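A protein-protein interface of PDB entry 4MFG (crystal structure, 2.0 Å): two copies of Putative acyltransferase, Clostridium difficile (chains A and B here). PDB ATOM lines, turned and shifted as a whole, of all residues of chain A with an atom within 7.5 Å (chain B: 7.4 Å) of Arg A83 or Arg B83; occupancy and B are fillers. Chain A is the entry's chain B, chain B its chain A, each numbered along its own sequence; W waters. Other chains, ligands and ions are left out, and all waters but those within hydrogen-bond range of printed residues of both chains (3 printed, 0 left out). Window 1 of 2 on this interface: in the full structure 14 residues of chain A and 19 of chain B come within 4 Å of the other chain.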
ATOM      1  N   TYR A  41      20.744  -2.102  33.579  1.00  0.00           N
ATOM      2  CA  TYR A  41      19.542  -2.913  33.769  1.00  0.00           C
ATOM      3  C   TYR A  41      19.734  -4.383  33.556  1.00  0.00           C
ATOM      4  O   TYR A  41      20.238  -4.828  32.544  1.00  0.00           O
ATOM      5  CB  TYR A  41      18.373  -2.389  32.917  1.00  0.00           C
ATOM      6  CG  TYR A  41      18.100  -0.943  33.229  1.00  0.00           C
ATOM      7  CD1 TYR A  41      17.264  -0.576  34.290  1.00  0.00           C
ATOM      8  CD2 TYR A  41      18.732   0.046  32.540  1.00  0.00           C
ATOM      9  CE1 TYR A  41      17.035   0.756  34.590  1.00  0.00           C
ATOM     10  CE2 TYR A  41      18.522   1.381  32.851  1.00  0.00           C
ATOM     11  CZ  TYR A  41      17.660   1.724  33.876  1.00  0.00           C
ATOM     12  OH  TYR A  41      17.450   3.063  34.170  1.00  0.00           O
ATOM     13  N   ILE A  60      29.136  -1.594  32.913  1.00  0.00           N
ATOM     14  CA  ILE A  60      28.689  -2.953  32.679  1.00  0.00           C
ATOM     15  C   ILE A  60      27.264  -2.821  32.164  1.00  0.00           C
ATOM     16  O   ILE A  60      26.358  -2.558  32.931  1.00  0.00           O
ATOM     17  CB  ILE A  60      28.714  -3.767  33.978  1.00  0.00           C
ATOM     18  CG1 ILE A  60      30.115  -3.718  34.599  1.00  0.00           C
ATOM     19  CG2 ILE A  60      28.238  -5.191  33.728  1.00  0.00           C
ATOM     20  CD1 ILE A  60      31.199  -4.325  33.737  1.00  0.00           C
ATOM     21  N   GLN A  61      27.061  -3.011  30.875  1.00  0.00           N
ATOM     22  CA  GLN A  61      25.750  -2.751  30.280  1.00  0.00           C
ATOM     23  C   GLN A  61      24.676  -3.816  30.506  1.00  0.00           C
ATOM     24  O   GLN A  61      24.924  -4.894  31.042  1.00  0.00           O
ATOM     25  CB  GLN A  61      25.888  -2.391  28.799  1.00  0.00           C
ATOM     26  CG  GLN A  61      26.735  -1.150  28.569  1.00  0.00           C
ATOM     27  CD  GLN A  61      26.960  -0.861  27.106  1.00  0.00           C
ATOM     28  OE1 GLN A  61      26.169  -1.229  26.244  1.00  0.00           O
ATOM     29  NE2 GLN A  61      28.033  -0.172  26.827  1.00  0.00           N
ATOM     30  N   ASP A  62      23.478  -3.466  30.082  1.00  0.00           N
ATOM     31  CA  ASP A  62      22.267  -4.243  30.338  1.00  0.00           C
ATOM     32  C   ASP A  62      22.420  -5.725  30.087  1.00  0.00           C
ATOM     33  O   ASP A  62      22.935  -6.151  29.076  1.00  0.00           O
ATOM     34  CB  ASP A  62      21.114  -3.707  29.501  1.00  0.00           C
ATOM     35  CG  ASP A  62      21.184  -2.220  29.328  1.00  0.00           C
ATOM     36  OD1 ASP A  62      21.985  -1.767  28.495  1.00  0.00           O
ATOM     37  OD2 ASP A  62      20.433  -1.513  29.990  1.00  0.00           O
ATOM     38  N   CYS A  63      22.014  -6.510  31.067  1.00  0.00           N
ATOM     39  CA  CYS A  63      21.999  -7.964  30.969  1.00  0.00           C
ATOM     40  C   CYS A  63      23.348  -8.610  30.834  1.00  0.00           C
ATOM     41  O   CYS A  63      23.401  -9.817  30.490  1.00  0.00           O
ATOM     42  CB  CYS A  63      21.109  -8.431  29.809  1.00  0.00           C
ATOM     43  SG  CYS A  63      19.383  -7.934  29.963  1.00  0.00           S
ATOM     44  N   SER A  64      24.420  -7.852  31.117  1.00  0.00           N
ATOM     45  CA  SER A  64      25.769  -8.424  31.088  1.00  0.00           C
ATOM     46  C   SER A  64      25.969  -9.228  32.360  1.00  0.00           C
ATOM     47  O   SER A  64      25.334  -8.975  33.392  1.00  0.00           O
ATOM     48  CB  SER A  64      26.844  -7.357  30.953  1.00  0.00           C
ATOM     49  OG  SER A  64      26.778  -6.735  29.671  1.00  0.00           O
ATOM     50  N   ILE A  65      26.839 -10.222  32.266  1.00  0.00           N
ATOM     51  CA  ILE A  65      27.106 -11.152  33.333  1.00  0.00           C
ATOM     52  C   ILE A  65      28.585 -11.243  33.643  1.00  0.00           C
ATOM     53  O   ILE A  65      29.406 -11.457  32.753  1.00  0.00           O
ATOM     54  CB  ILE A  65      26.612 -12.551  32.957  1.00  0.00           C
ATOM     55  CG1 ILE A  65      25.107 -12.534  32.778  1.00  0.00           C
ATOM     56  CG2 ILE A  65      26.929 -13.560  34.047  1.00  0.00           C
ATOM     57  CD1 ILE A  65      24.620 -13.798  32.156  1.00  0.00           C
ATOM     58  N   VAL A  80      31.627  -2.582  28.820  1.00  0.00           N
ATOM     59  CA  VAL A  80      31.208  -3.945  28.585  1.00  0.00           C
ATOM     60  C   VAL A  80      29.878  -3.835  27.908  1.00  0.00           C
ATOM     61  O   VAL A  80      28.905  -3.459  28.525  1.00  0.00           O
ATOM     62  CB  VAL A  80      31.114  -4.766  29.876  1.00  0.00           C
ATOM     63  CG1 VAL A  80      30.447  -6.105  29.624  1.00  0.00           C
ATOM     64  CG2 VAL A  80      32.490  -4.961  30.468  1.00  0.00           C
ATOM     65  N   GLY A  81      29.840  -4.133  26.613  1.00  0.00           N
ATOM     66  CA  GLY A  81      28.602  -4.060  25.831  1.00  0.00           C
ATOM     67  C   GLY A  81      27.432  -4.923  26.263  1.00  0.00           C
ATOM     68  O   GLY A  81      27.597  -5.958  26.901  1.00  0.00           O
ATOM     69  N   HIS A  82      26.244  -4.518  25.845  1.00  0.00           N
ATOM     70  CA  HIS A  82      25.023  -5.209  26.225  1.00  0.00           C
ATOM     71  C   HIS A  82      25.134  -6.741  26.176  1.00  0.00           C
ATOM     72  O   HIS A  82      25.597  -7.316  25.219  1.00  0.00           O
ATOM     73  CB  HIS A  82      23.849  -4.844  25.289  1.00  0.00           C
ATOM     74  CG  HIS A  82      23.640  -3.385  25.081  1.00  0.00           C
ATOM     75  ND1 HIS A  82      23.051  -2.565  26.014  1.00  0.00           N
ATOM     76  CD2 HIS A  82      23.860  -2.614  23.994  1.00  0.00           C
ATOM     77  CE1 HIS A  82      22.972  -1.339  25.529  1.00  0.00           C
ATOM     78  NE2 HIS A  82      23.481  -1.338  24.315  1.00  0.00           N
ATOM     79  N   ARG A  83      24.687  -7.404  27.222  1.00  0.00           N
ATOM     80  CA  ARG A  83      24.577  -8.858  27.157  1.00  0.00           C
ATOM     81  C   ARG A  83      25.899  -9.575  26.893  1.00  0.00           C
ATOM     82  O   ARG A  83      25.923 -10.675  26.255  1.00  0.00           O
ATOM     83  CB  ARG A  83      23.592  -9.257  26.013  1.00  0.00           C
ATOM     84  CG  ARG A  83      22.594 -10.258  26.490  1.00  0.00           C
ATOM     85  CD  ARG A  83      22.346 -11.443  25.598  1.00  0.00           C
ATOM     86  NE  ARG A  83      21.904 -11.278  24.220  1.00  0.00           N
ATOM     87  CZ  ARG A  83      22.620 -11.666  23.154  1.00  0.00           C
ATOM     88  NH1 ARG A  83      23.850 -12.178  23.310  1.00  0.00           N
ATOM     89  NH2 ARG A  83      22.115 -11.538  21.923  1.00  0.00           N
ATOM     90  N   SER A  84      27.000  -8.985  27.347  1.00  0.00           N
ATOM     91  CA  SER A  84      28.280  -9.644  27.211  1.00  0.00           C
ATOM     92  C   SER A  84      28.495 -10.510  28.432  1.00  0.00           C
ATOM     93  O   SER A  84      27.868 -10.317  29.479  1.00  0.00           O
ATOM     94  CB  SER A  84      29.405  -8.612  27.106  1.00  0.00           C
ATOM     95  OG  SER A  84      29.238  -7.796  25.944  1.00  0.00           O
ATOM     96  N   ILE A  85      29.345 -11.505  28.294  1.00  0.00           N
ATOM     97  CA  ILE A  85      29.751 -12.339  29.429  1.00  0.00           C
ATOM     98  C   ILE A  85      31.272 -12.215  29.608  1.00  0.00           C
ATOM     99  O   ILE A  85      32.039 -12.601  28.725  1.00  0.00           O
ATOM    100  CB  ILE A  85      29.435 -13.815  29.241  1.00  0.00           C
ATOM    101  CG1 ILE A  85      27.982 -14.012  28.785  1.00  0.00           C
ATOM    102  CG2 ILE A  85      29.734 -14.564  30.548  1.00  0.00           C
ATOM    103  CD1 ILE A  85      27.583 -15.480  28.710  1.00  0.00           C
ATOM    104  N   VAL A  86      31.688 -11.638  30.738  1.00  0.00           N
ATOM    105  CA  VAL A  86      33.090 -11.474  31.102  1.00  0.00           C
ATOM    106  C   VAL A  86      33.328 -12.468  32.219  1.00  0.00           C
ATOM    107  O   VAL A  86      32.967 -12.213  33.349  1.00  0.00           O
ATOM    108  CB  VAL A  86      33.334 -10.059  31.589  1.00  0.00           C
ATOM    109  CG1 VAL A  86      34.807  -9.834  31.871  1.00  0.00           C
ATOM    110  CG2 VAL A  86      32.837  -9.052  30.565  1.00  0.00           C
ATOM    111  N   GLY A  98      32.531  -5.464  22.633  1.00  0.00           N
ATOM    112  CA  GLY A  98      31.325  -5.436  21.774  1.00  0.00           C
ATOM    113  C   GLY A  98      30.160  -6.253  22.331  1.00  0.00           C
ATOM    114  O   GLY A  98      30.366  -7.332  22.878  1.00  0.00           O
ATOM    115  N   MET A  99      28.936  -5.734  22.147  1.00  0.00           N
ATOM    116  CA  MET A  99      27.734  -6.345  22.687  1.00  0.00           C
ATOM    117  C   MET A  99      27.644  -7.816  22.281  1.00  0.00           C
ATOM    118  O   MET A  99      27.983  -8.231  21.173  1.00  0.00           O
ATOM    119  CB  MET A  99      26.471  -5.536  22.331  1.00  0.00           C
ATOM    120  CG  MET A  99      26.122  -5.512  20.862  1.00  0.00           C
ATOM    121  SD  MET A  99      24.759  -4.442  20.342  1.00  0.00           S
ATOM    122  CE  MET A  99      25.643  -2.884  20.303  1.00  0.00           C
ATOM    123  N   GLY A 100      27.228  -8.599  23.232  1.00  0.00           N
ATOM    124  CA  GLY A 100      27.046 -10.038  23.025  1.00  0.00           C
ATOM    125  C   GLY A 100      28.292 -10.869  23.029  1.00  0.00           C
ATOM    126  O   GLY A 100      28.235 -12.052  22.720  1.00  0.00           O
ATOM    127  N   SER A 101      29.418 -10.289  23.416  1.00  0.00           N
ATOM    128  CA  SER A 101      30.681 -11.033  23.389  1.00  0.00           C
ATOM    129  C   SER A 101      30.814 -11.901  24.629  1.00  0.00           C
ATOM    130  O   SER A 101      30.186 -11.647  25.646  1.00  0.00           O
ATOM    131  CB  SER A 101      31.870 -10.070  23.303  1.00  0.00           C
ATOM    132  OG  SER A 101      31.847  -9.330  22.071  1.00  0.00           O
ATOM    133  N   ILE A 102      31.611 -12.942  24.516  1.00  0.00           N
ATOM    134  CA  ILE A 102      31.889 -13.836  25.622  1.00  0.00           C
ATOM    135  C   ILE A 102      33.394 -13.939  25.698  1.00  0.00           C
ATOM    136  O   ILE A 102      34.038 -14.207  24.694  1.00  0.00           O
ATOM    137  CB  ILE A 102      31.318 -15.221  25.394  1.00  0.00           C
ATOM    138  CG1 ILE A 102      29.794 -15.141  25.345  1.00  0.00           C
ATOM    139  CG2 ILE A 102      31.746 -16.153  26.518  1.00  0.00           C
ATOM    140  CD1 ILE A 102      29.135 -16.404  24.828  1.00  0.00           C
ATOM    141  N   GLY A 118      29.481  -9.816  19.463  1.00  0.00           N
ATOM    142  CA  GLY A 118      29.345 -11.286  19.363  1.00  0.00           C
ATOM    143  C   GLY A 118      30.621 -12.099  19.266  1.00  0.00           C
ATOM    144  O   GLY A 118      30.579 -13.246  18.824  1.00  0.00           O
ATOM    145  N   ILE B  60       8.415  -8.478  22.210  1.00  0.00           N
ATOM    146  CA  ILE B  60       9.828  -8.412  22.588  1.00  0.00           C
ATOM    147  C   ILE B  60       9.990  -9.464  23.656  1.00  0.00           C
ATOM    148  O   ILE B  60       9.594  -9.289  24.804  1.00  0.00           O
ATOM    149  CB  ILE B  60      10.175  -7.034  23.150  1.00  0.00           C
ATOM    150  CG1 ILE B  60       9.767  -5.947  22.167  1.00  0.00           C
ATOM    151  CG2 ILE B  60      11.651  -6.933  23.434  1.00  0.00           C
ATOM    152  CD1 ILE B  60      10.545  -5.920  20.884  1.00  0.00           C
ATOM    153  N   GLN B  61      10.570 -10.573  23.284  1.00  0.00           N
ATOM    154  CA  GLN B  61      10.649 -11.682  24.205  1.00  0.00           C
ATOM    155  C   GLN B  61      11.661 -11.512  25.344  1.00  0.00           C
ATOM    156  O   GLN B  61      12.382 -10.515  25.409  1.00  0.00           O
ATOM    157  CB  GLN B  61      10.820 -12.987  23.419  1.00  0.00           C
ATOM    158  CG  GLN B  61       9.665 -13.217  22.472  1.00  0.00           C
ATOM    159  CD  GLN B  61       9.791 -14.482  21.627  1.00  0.00           C
ATOM    160  OE1 GLN B  61      10.529 -15.405  21.950  1.00  0.00           O
ATOM    161  NE2 GLN B  61       9.035 -14.528  20.563  1.00  0.00           N
ATOM    162  N   ASP B  62      11.668 -12.508  26.248  1.00  0.00           N
ATOM    163  CA  ASP B  62      12.441 -12.485  27.474  1.00  0.00           C
ATOM    164  C   ASP B  62      13.905 -12.145  27.258  1.00  0.00           C
ATOM    165  O   ASP B  62      14.535 -12.613  26.327  1.00  0.00           O
ATOM    166  CB  ASP B  62      12.320 -13.838  28.180  1.00  0.00           C
ATOM    167  CG  ASP B  62      10.974 -14.449  27.984  1.00  0.00           C
ATOM    168  OD1 ASP B  62      10.742 -15.038  26.912  1.00  0.00           O
ATOM    169  OD2 ASP B  62      10.118 -14.327  28.878  1.00  0.00           O
ATOM    170  N   CYS B  63      14.410 -11.263  28.116  1.00  0.00           N
ATOM    171  CA  CYS B  63      15.784 -10.772  28.118  1.00  0.00           C
ATOM    172  C   CYS B  63      16.252 -10.132  26.798  1.00  0.00           C
ATOM    173  O   CYS B  63      17.436  -9.993  26.592  1.00  0.00           O
ATOM    174  CB  CYS B  63      16.757 -11.870  28.545  1.00  0.00           C
ATOM    175  SG  CYS B  63      16.152 -12.802  29.941  1.00  0.00           S
ATOM    176  N   SER B  64      15.336  -9.770  25.898  1.00  0.00           N
ATOM    177  CA  SER B  64      15.773  -9.016  24.713  1.00  0.00           C
ATOM    178  C   SER B  64      16.199  -7.618  25.139  1.00  0.00           C
ATOM    179  O   SER B  64      15.840  -7.147  26.213  1.00  0.00           O
ATOM    180  CB  SER B  64      14.707  -8.942  23.637  1.00  0.00           C
ATOM    181  OG  SER B  64      14.522 -10.196  23.019  1.00  0.00           O
ATOM    182  N   ILE B  65      17.007  -6.972  24.306  1.00  0.00           N
ATOM    183  CA  ILE B  65      17.513  -5.634  24.568  1.00  0.00           C
ATOM    184  C   ILE B  65      17.342  -4.773  23.337  1.00  0.00           C
ATOM    185  O   ILE B  65      17.708  -5.178  22.235  1.00  0.00           O
ATOM    186  CB  ILE B  65      18.996  -5.681  24.880  1.00  0.00           C
ATOM    187  CG1 ILE B  65      19.201  -6.420  26.167  1.00  0.00           C
ATOM    188  CG2 ILE B  65      19.575  -4.280  25.053  1.00  0.00           C
ATOM    189  CD1 ILE B  65      20.585  -6.957  26.282  1.00  0.00           C
ATOM    190  N   VAL B  80      10.371 -10.489  18.246  1.00  0.00           N
ATOM    191  CA  VAL B  80      11.776 -10.414  18.620  1.00  0.00           C
ATOM    192  C   VAL B  80      12.011 -11.627  19.551  1.00  0.00           C
ATOM    193  O   VAL B  80      11.540 -11.675  20.695  1.00  0.00           O
ATOM    194  CB  VAL B  80      12.154  -9.079  19.285  1.00  0.00           C
ATOM    195  CG1 VAL B  80      13.630  -9.041  19.589  1.00  0.00           C
ATOM    196  CG2 VAL B  80      11.818  -7.922  18.340  1.00  0.00           C
ATOM    197  N   GLY B  81      12.719 -12.623  19.025  1.00  0.00           N
ATOM    198  CA  GLY B  81      12.939 -13.871  19.759  1.00  0.00           C
ATOM    199  C   GLY B  81      13.719 -13.667  21.017  1.00  0.00           C
ATOM    200  O   GLY B  81      14.463 -12.695  21.124  1.00  0.00           O
ATOM    201  N   HIS B  82      13.602 -14.634  21.932  1.00  0.00           N
ATOM    202  CA  HIS B  82      14.299 -14.589  23.217  1.00  0.00           C
ATOM    203  C   HIS B  82      15.728 -14.095  23.101  1.00  0.00           C
ATOM    204  O   HIS B  82      16.461 -14.517  22.212  1.00  0.00           O
ATOM    205  CB  HIS B  82      14.350 -15.997  23.868  1.00  0.00           C
ATOM    206  CG  HIS B  82      13.038 -16.715  23.874  1.00  0.00           C
ATOM    207  ND1 HIS B  82      12.088 -16.530  24.862  1.00  0.00           N
ATOM    208  CD2 HIS B  82      12.521 -17.629  23.020  1.00  0.00           C
ATOM    209  CE1 HIS B  82      11.051 -17.312  24.624  1.00  0.00           C
ATOM    210  NE2 HIS B  82      11.277 -17.971  23.501  1.00  0.00           N
ATOM    211  N   ARG B  83      16.142 -13.230  24.028  1.00  0.00           N
ATOM    212  CA  ARG B  83      17.516 -12.774  24.067  1.00  0.00           C
ATOM    213  C   ARG B  83      18.104 -12.152  22.829  1.00  0.00           C
ATOM    214  O   ARG B  83      19.302 -12.320  22.588  1.00  0.00           O
ATOM    215  CB  ARG B  83      18.453 -13.952  24.383  1.00  0.00           C
ATOM    216  CG  ARG B  83      19.000 -13.897  25.769  1.00  0.00           C
ATOM    217  CD  ARG B  83      20.484 -14.175  25.792  1.00  0.00           C
ATOM    218  NE  ARG B  83      20.964 -15.541  25.578  1.00  0.00           N
ATOM    219  CZ  ARG B  83      21.596 -15.984  24.480  1.00  0.00           C
ATOM    220  NH1 ARG B  83      21.769 -15.213  23.416  1.00  0.00           N
ATOM    221  NH2 ARG B  83      22.054 -17.230  24.443  1.00  0.00           N
ATOM    222  N   SER B  84      17.302 -11.509  22.009  1.00  0.00           N
ATOM    223  CA  SER B  84      17.867 -10.871  20.830  1.00  0.00           C
ATOM    224  C   SER B  84      18.303  -9.478  21.246  1.00  0.00           C
ATOM    225  O   SER B  84      17.819  -8.944  22.242  1.00  0.00           O
ATOM    226  CB  SER B  84      16.832 -10.767  19.721  1.00  0.00           C
ATOM    227  OG  SER B  84      16.333 -12.060  19.361  1.00  0.00           O
ATOM    228  N   ILE B  85      19.230  -8.909  20.492  1.00  0.00           N
ATOM    229  CA  ILE B  85      19.647  -7.532  20.651  1.00  0.00           C
ATOM    230  C   ILE B  85      19.338  -6.794  19.364  1.00  0.00           C
ATOM    231  O   ILE B  85      19.898  -7.099  18.316  1.00  0.00           O
ATOM    232  CB  ILE B  85      21.151  -7.347  20.881  1.00  0.00           C
ATOM    233  CG1 ILE B  85      21.641  -8.181  22.073  1.00  0.00           C
ATOM    234  CG2 ILE B  85      21.437  -5.864  21.138  1.00  0.00           C
ATOM    235  CD1 ILE B  85      23.109  -7.923  22.401  1.00  0.00           C
ATOM    236  N   VAL B  86      18.458  -5.806  19.457  1.00  0.00           N
ATOM    237  CA  VAL B  86      18.052  -4.985  18.323  1.00  0.00           C
ATOM    238  C   VAL B  86      18.599  -3.597  18.599  1.00  0.00           C
ATOM    239  O   VAL B  86      18.067  -2.860  19.447  1.00  0.00           O
ATOM    240  CB  VAL B  86      16.543  -4.934  18.235  1.00  0.00           C
ATOM    241  CG1 VAL B  86      16.132  -4.171  16.999  1.00  0.00           C
ATOM    242  CG2 VAL B  86      15.973  -6.346  18.223  1.00  0.00           C
ATOM    243  N   GLY B  98      15.003 -14.501  14.953  1.00  0.00           N
ATOM    244  CA  GLY B  98      15.334 -15.742  15.674  1.00  0.00           C
ATOM    245  C   GLY B  98      16.001 -15.437  17.001  1.00  0.00           C
ATOM    246  O   GLY B  98      16.785 -14.506  17.102  1.00  0.00           O
ATOM    247  N   MET B  99      15.713 -16.260  18.005  1.00  0.00           N
ATOM    248  CA  MET B  99      16.181 -16.036  19.364  1.00  0.00           C
ATOM    249  C   MET B  99      17.695 -15.936  19.344  1.00  0.00           C
ATOM    250  O   MET B  99      18.366 -16.573  18.546  1.00  0.00           O
ATOM    251  CB  MET B  99      15.648 -17.129  20.334  1.00  0.00           C
ATOM    252  CG  MET B  99      16.312 -18.478  20.156  1.00  0.00           C
ATOM    253  SD  MET B  99      15.431 -19.867  20.884  1.00  0.00           S
ATOM    254  CE  MET B  99      13.982 -19.963  19.851  1.00  0.00           C
ATOM    255  N   GLY B 100      18.216 -15.085  20.217  1.00  0.00           N
ATOM    256  CA  GLY B 100      19.639 -14.839  20.316  1.00  0.00           C
ATOM    257  C   GLY B 100      20.321 -14.089  19.184  1.00  0.00           C
ATOM    258  O   GLY B 100      21.530 -14.118  19.100  1.00  0.00           O
ATOM    259  N   SER B 101      19.574 -13.457  18.285  1.00  0.00           N
ATOM    260  CA  SER B 101      20.168 -12.726  17.191  1.00  0.00           C
ATOM    261  C   SER B 101      20.610 -11.336  17.636  1.00  0.00           C
ATOM    262  O   SER B 101      20.090 -10.802  18.622  1.00  0.00           O
ATOM    263  CB  SER B 101      19.185 -12.583  16.030  1.00  0.00           C
ATOM    264  OG  SER B 101      18.814 -13.845  15.473  1.00  0.00           O
ATOM    265  N   ILE B 102      21.532 -10.742  16.876  1.00  0.00           N
ATOM    266  CA  ILE B 102      22.058  -9.396  17.133  1.00  0.00           C
ATOM    267  C   ILE B 102      22.030  -8.599  15.840  1.00  0.00           C
ATOM    268  O   ILE B 102      22.680  -8.980  14.836  1.00  0.00           O
ATOM    269  CB  ILE B 102      23.514  -9.426  17.633  1.00  0.00           C
ATOM    270  CG1 ILE B 102      23.597 -10.024  19.033  1.00  0.00           C
ATOM    271  CG2 ILE B 102      24.080  -8.010  17.719  1.00  0.00           C
ATOM    272  CD1 ILE B 102      25.003 -10.485  19.442  1.00  0.00           C
ATOM    273  N   ILE B 103      21.245  -7.535  15.831  1.00  0.00           N
ATOM    274  CA  ILE B 103      21.152  -6.674  14.629  1.00  0.00           C
ATOM    275  C   ILE B 103      21.597  -5.269  14.991  1.00  0.00           C
ATOM    276  O   ILE B 103      20.974  -4.599  15.839  1.00  0.00           O
ATOM    277  CB  ILE B 103      19.751  -6.636  14.068  1.00  0.00           C
ATOM    278  CG1 ILE B 103      19.248  -8.075  13.871  1.00  0.00           C
ATOM    279  CG2 ILE B 103      19.761  -5.874  12.753  1.00  0.00           C
ATOM    280  CD1 ILE B 103      17.826  -8.165  13.419  1.00  0.00           C
ATOM    281  N   GLY B 118      20.357 -16.996  16.544  1.00  0.00           N
ATOM    282  CA  GLY B 118      21.786 -16.755  16.650  1.00  0.00           C
ATOM    283  C   GLY B 118      22.464 -15.983  15.534  1.00  0.00           C
ATOM    284  O   GLY B 118      23.699 -15.996  15.440  1.00  0.00           O
ATOM    285  N   THR B 119      21.668 -15.284  14.722  1.00  0.00           N
ATOM    286  CA  THR B 119      22.182 -14.508  13.608  1.00  0.00           C
ATOM    287  C   THR B 119      22.856 -13.187  14.057  1.00  0.00           C
ATOM    288  O   THR B 119      22.371 -12.503  14.955  1.00  0.00           O
ATOM    289  CB  THR B 119      21.034 -14.185  12.600  1.00  0.00           C
ATOM    290  OG1 THR B 119      20.497 -15.402  12.076  1.00  0.00           O
ATOM    291  CG2 THR B 119      21.499 -13.318  11.465  1.00  0.00           C
HETATM  292  O   HOH W   1      23.416 -13.926  21.141  1.00  0.00           O
HETATM  293  O   HOH W   2      19.757  -9.728  25.005  1.00  0.00           O
HETATM  294  O   HOH W   3      18.255 -10.509  31.367  1.00  0.00           O
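Among the printed residues, merely in contact across the chains: Asp A62 with Ile B65, Cys A63 with Ile B65, His A82 with Ile B65, His A82 with Ile B85, Arg A83 with Ile B65, Arg A83 with Ile B85, Arg A83 with Gly B100, Arg A83 with Ser B101, Arg A83 with Ile B102 and Met A99 with Ile B85.
His A82 touches Ile B85, but with the chains exchanged Ile A85 does not touch His B82 (12.9 Å). Arg A83 touches Ile B65, but with the chains exchanged Ile A65 does not touch Arg B83 (7.6 Å). Arg A83 touches Gly B100, but with the chains exchanged Gly A100 does not touch Arg B83 (7.2 Å). Arg A83 touches Ser B101, but with the chains exchanged Ser A101 does not touch Arg B83 (9.1 Å).
Of the 20 printed residues of chain A, 5 touch a printed residue of chain B. Hydrophobic or aromatic side chains of chain A within 4 Å of the printed part of chain B: His A82 and Met A99. Printed residues of chain B that touch a printed residue of chain A: Ile B65, Arg B83, Ile B85, Gly B100, Ser B101 and Ile B102. Hydrophobic or aromatic side chains of chain B that line the printed part of chain A: Ile B65, Ile B85 and Ile B102. Among the printed residues, no Asp or Glu carboxylate lies within 4 Å of a Lys or Arg side-chain nitrogen of the other chain.
Water W2 lies within hydrogen-bond range of NE of Arg A83, O of Cys B63 and O of Ser B84. Water W1 lies within hydrogen-bond range of O of Gly B100 (2.8 Å), NH1 of Arg A83 (2.8 Å) and NH1 of Arg B83 (3.1 Å). Water W3 lies within hydrogen-bond range of the side-chain sulfur (SG) of Cys A63 (3.1 Å) and the side-chain sulfur (SG) of Cys B63 (3.4 Å).
The backbone carbonyl oxygen (O) of Arg B83 is in hydrogen-bond range of the guanidinium group (NH2) of Arg A83, at 3.0 Å.
N of Ile B102 is in hydrogen-bond range of O of Thr B119 (2.7 Å). N of Ile B103 sits at hydrogen-bond distance from O of Ile B85 (2.9 Å). N of Ile B85 is in hydrogen-bond range of O of Ser B101, at 2.8 Å. N of Ile B65 sits at hydrogen-bond distance from O of Ser B84 (3.0 Å). N of Cys A63 is in hydrogen-bond range of O of Tyr A41 (2.9 Å). The side-chain hydroxyl of Ser A64 sits at hydrogen-bond distance from the backbone NH of Arg A83 (3.3 Å).
Of chain B, only Ile B65, Arg B83, Ile B85, Gly B100, Ser B101 and Ile B102 come within 4 Å of Arg A83. Arg B83 touches just one residue of chain A: Arg A83. Of the printed residues of chain A, Ser B101 touches Arg A83 (3.9 Å). Of the printed residues of chain B, His A82 touches Ile B65 and Ile B85. The nearest residue of chain B that does not touch Arg A83 is Ser B84 (4.4 Å). The nearest residue of chain A that does not touch Arg B83 is Cys A63 (7.0 Å). The nearest printed residue of chain A that does not touch Ser B101 is Met A99 (8.1 Å).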
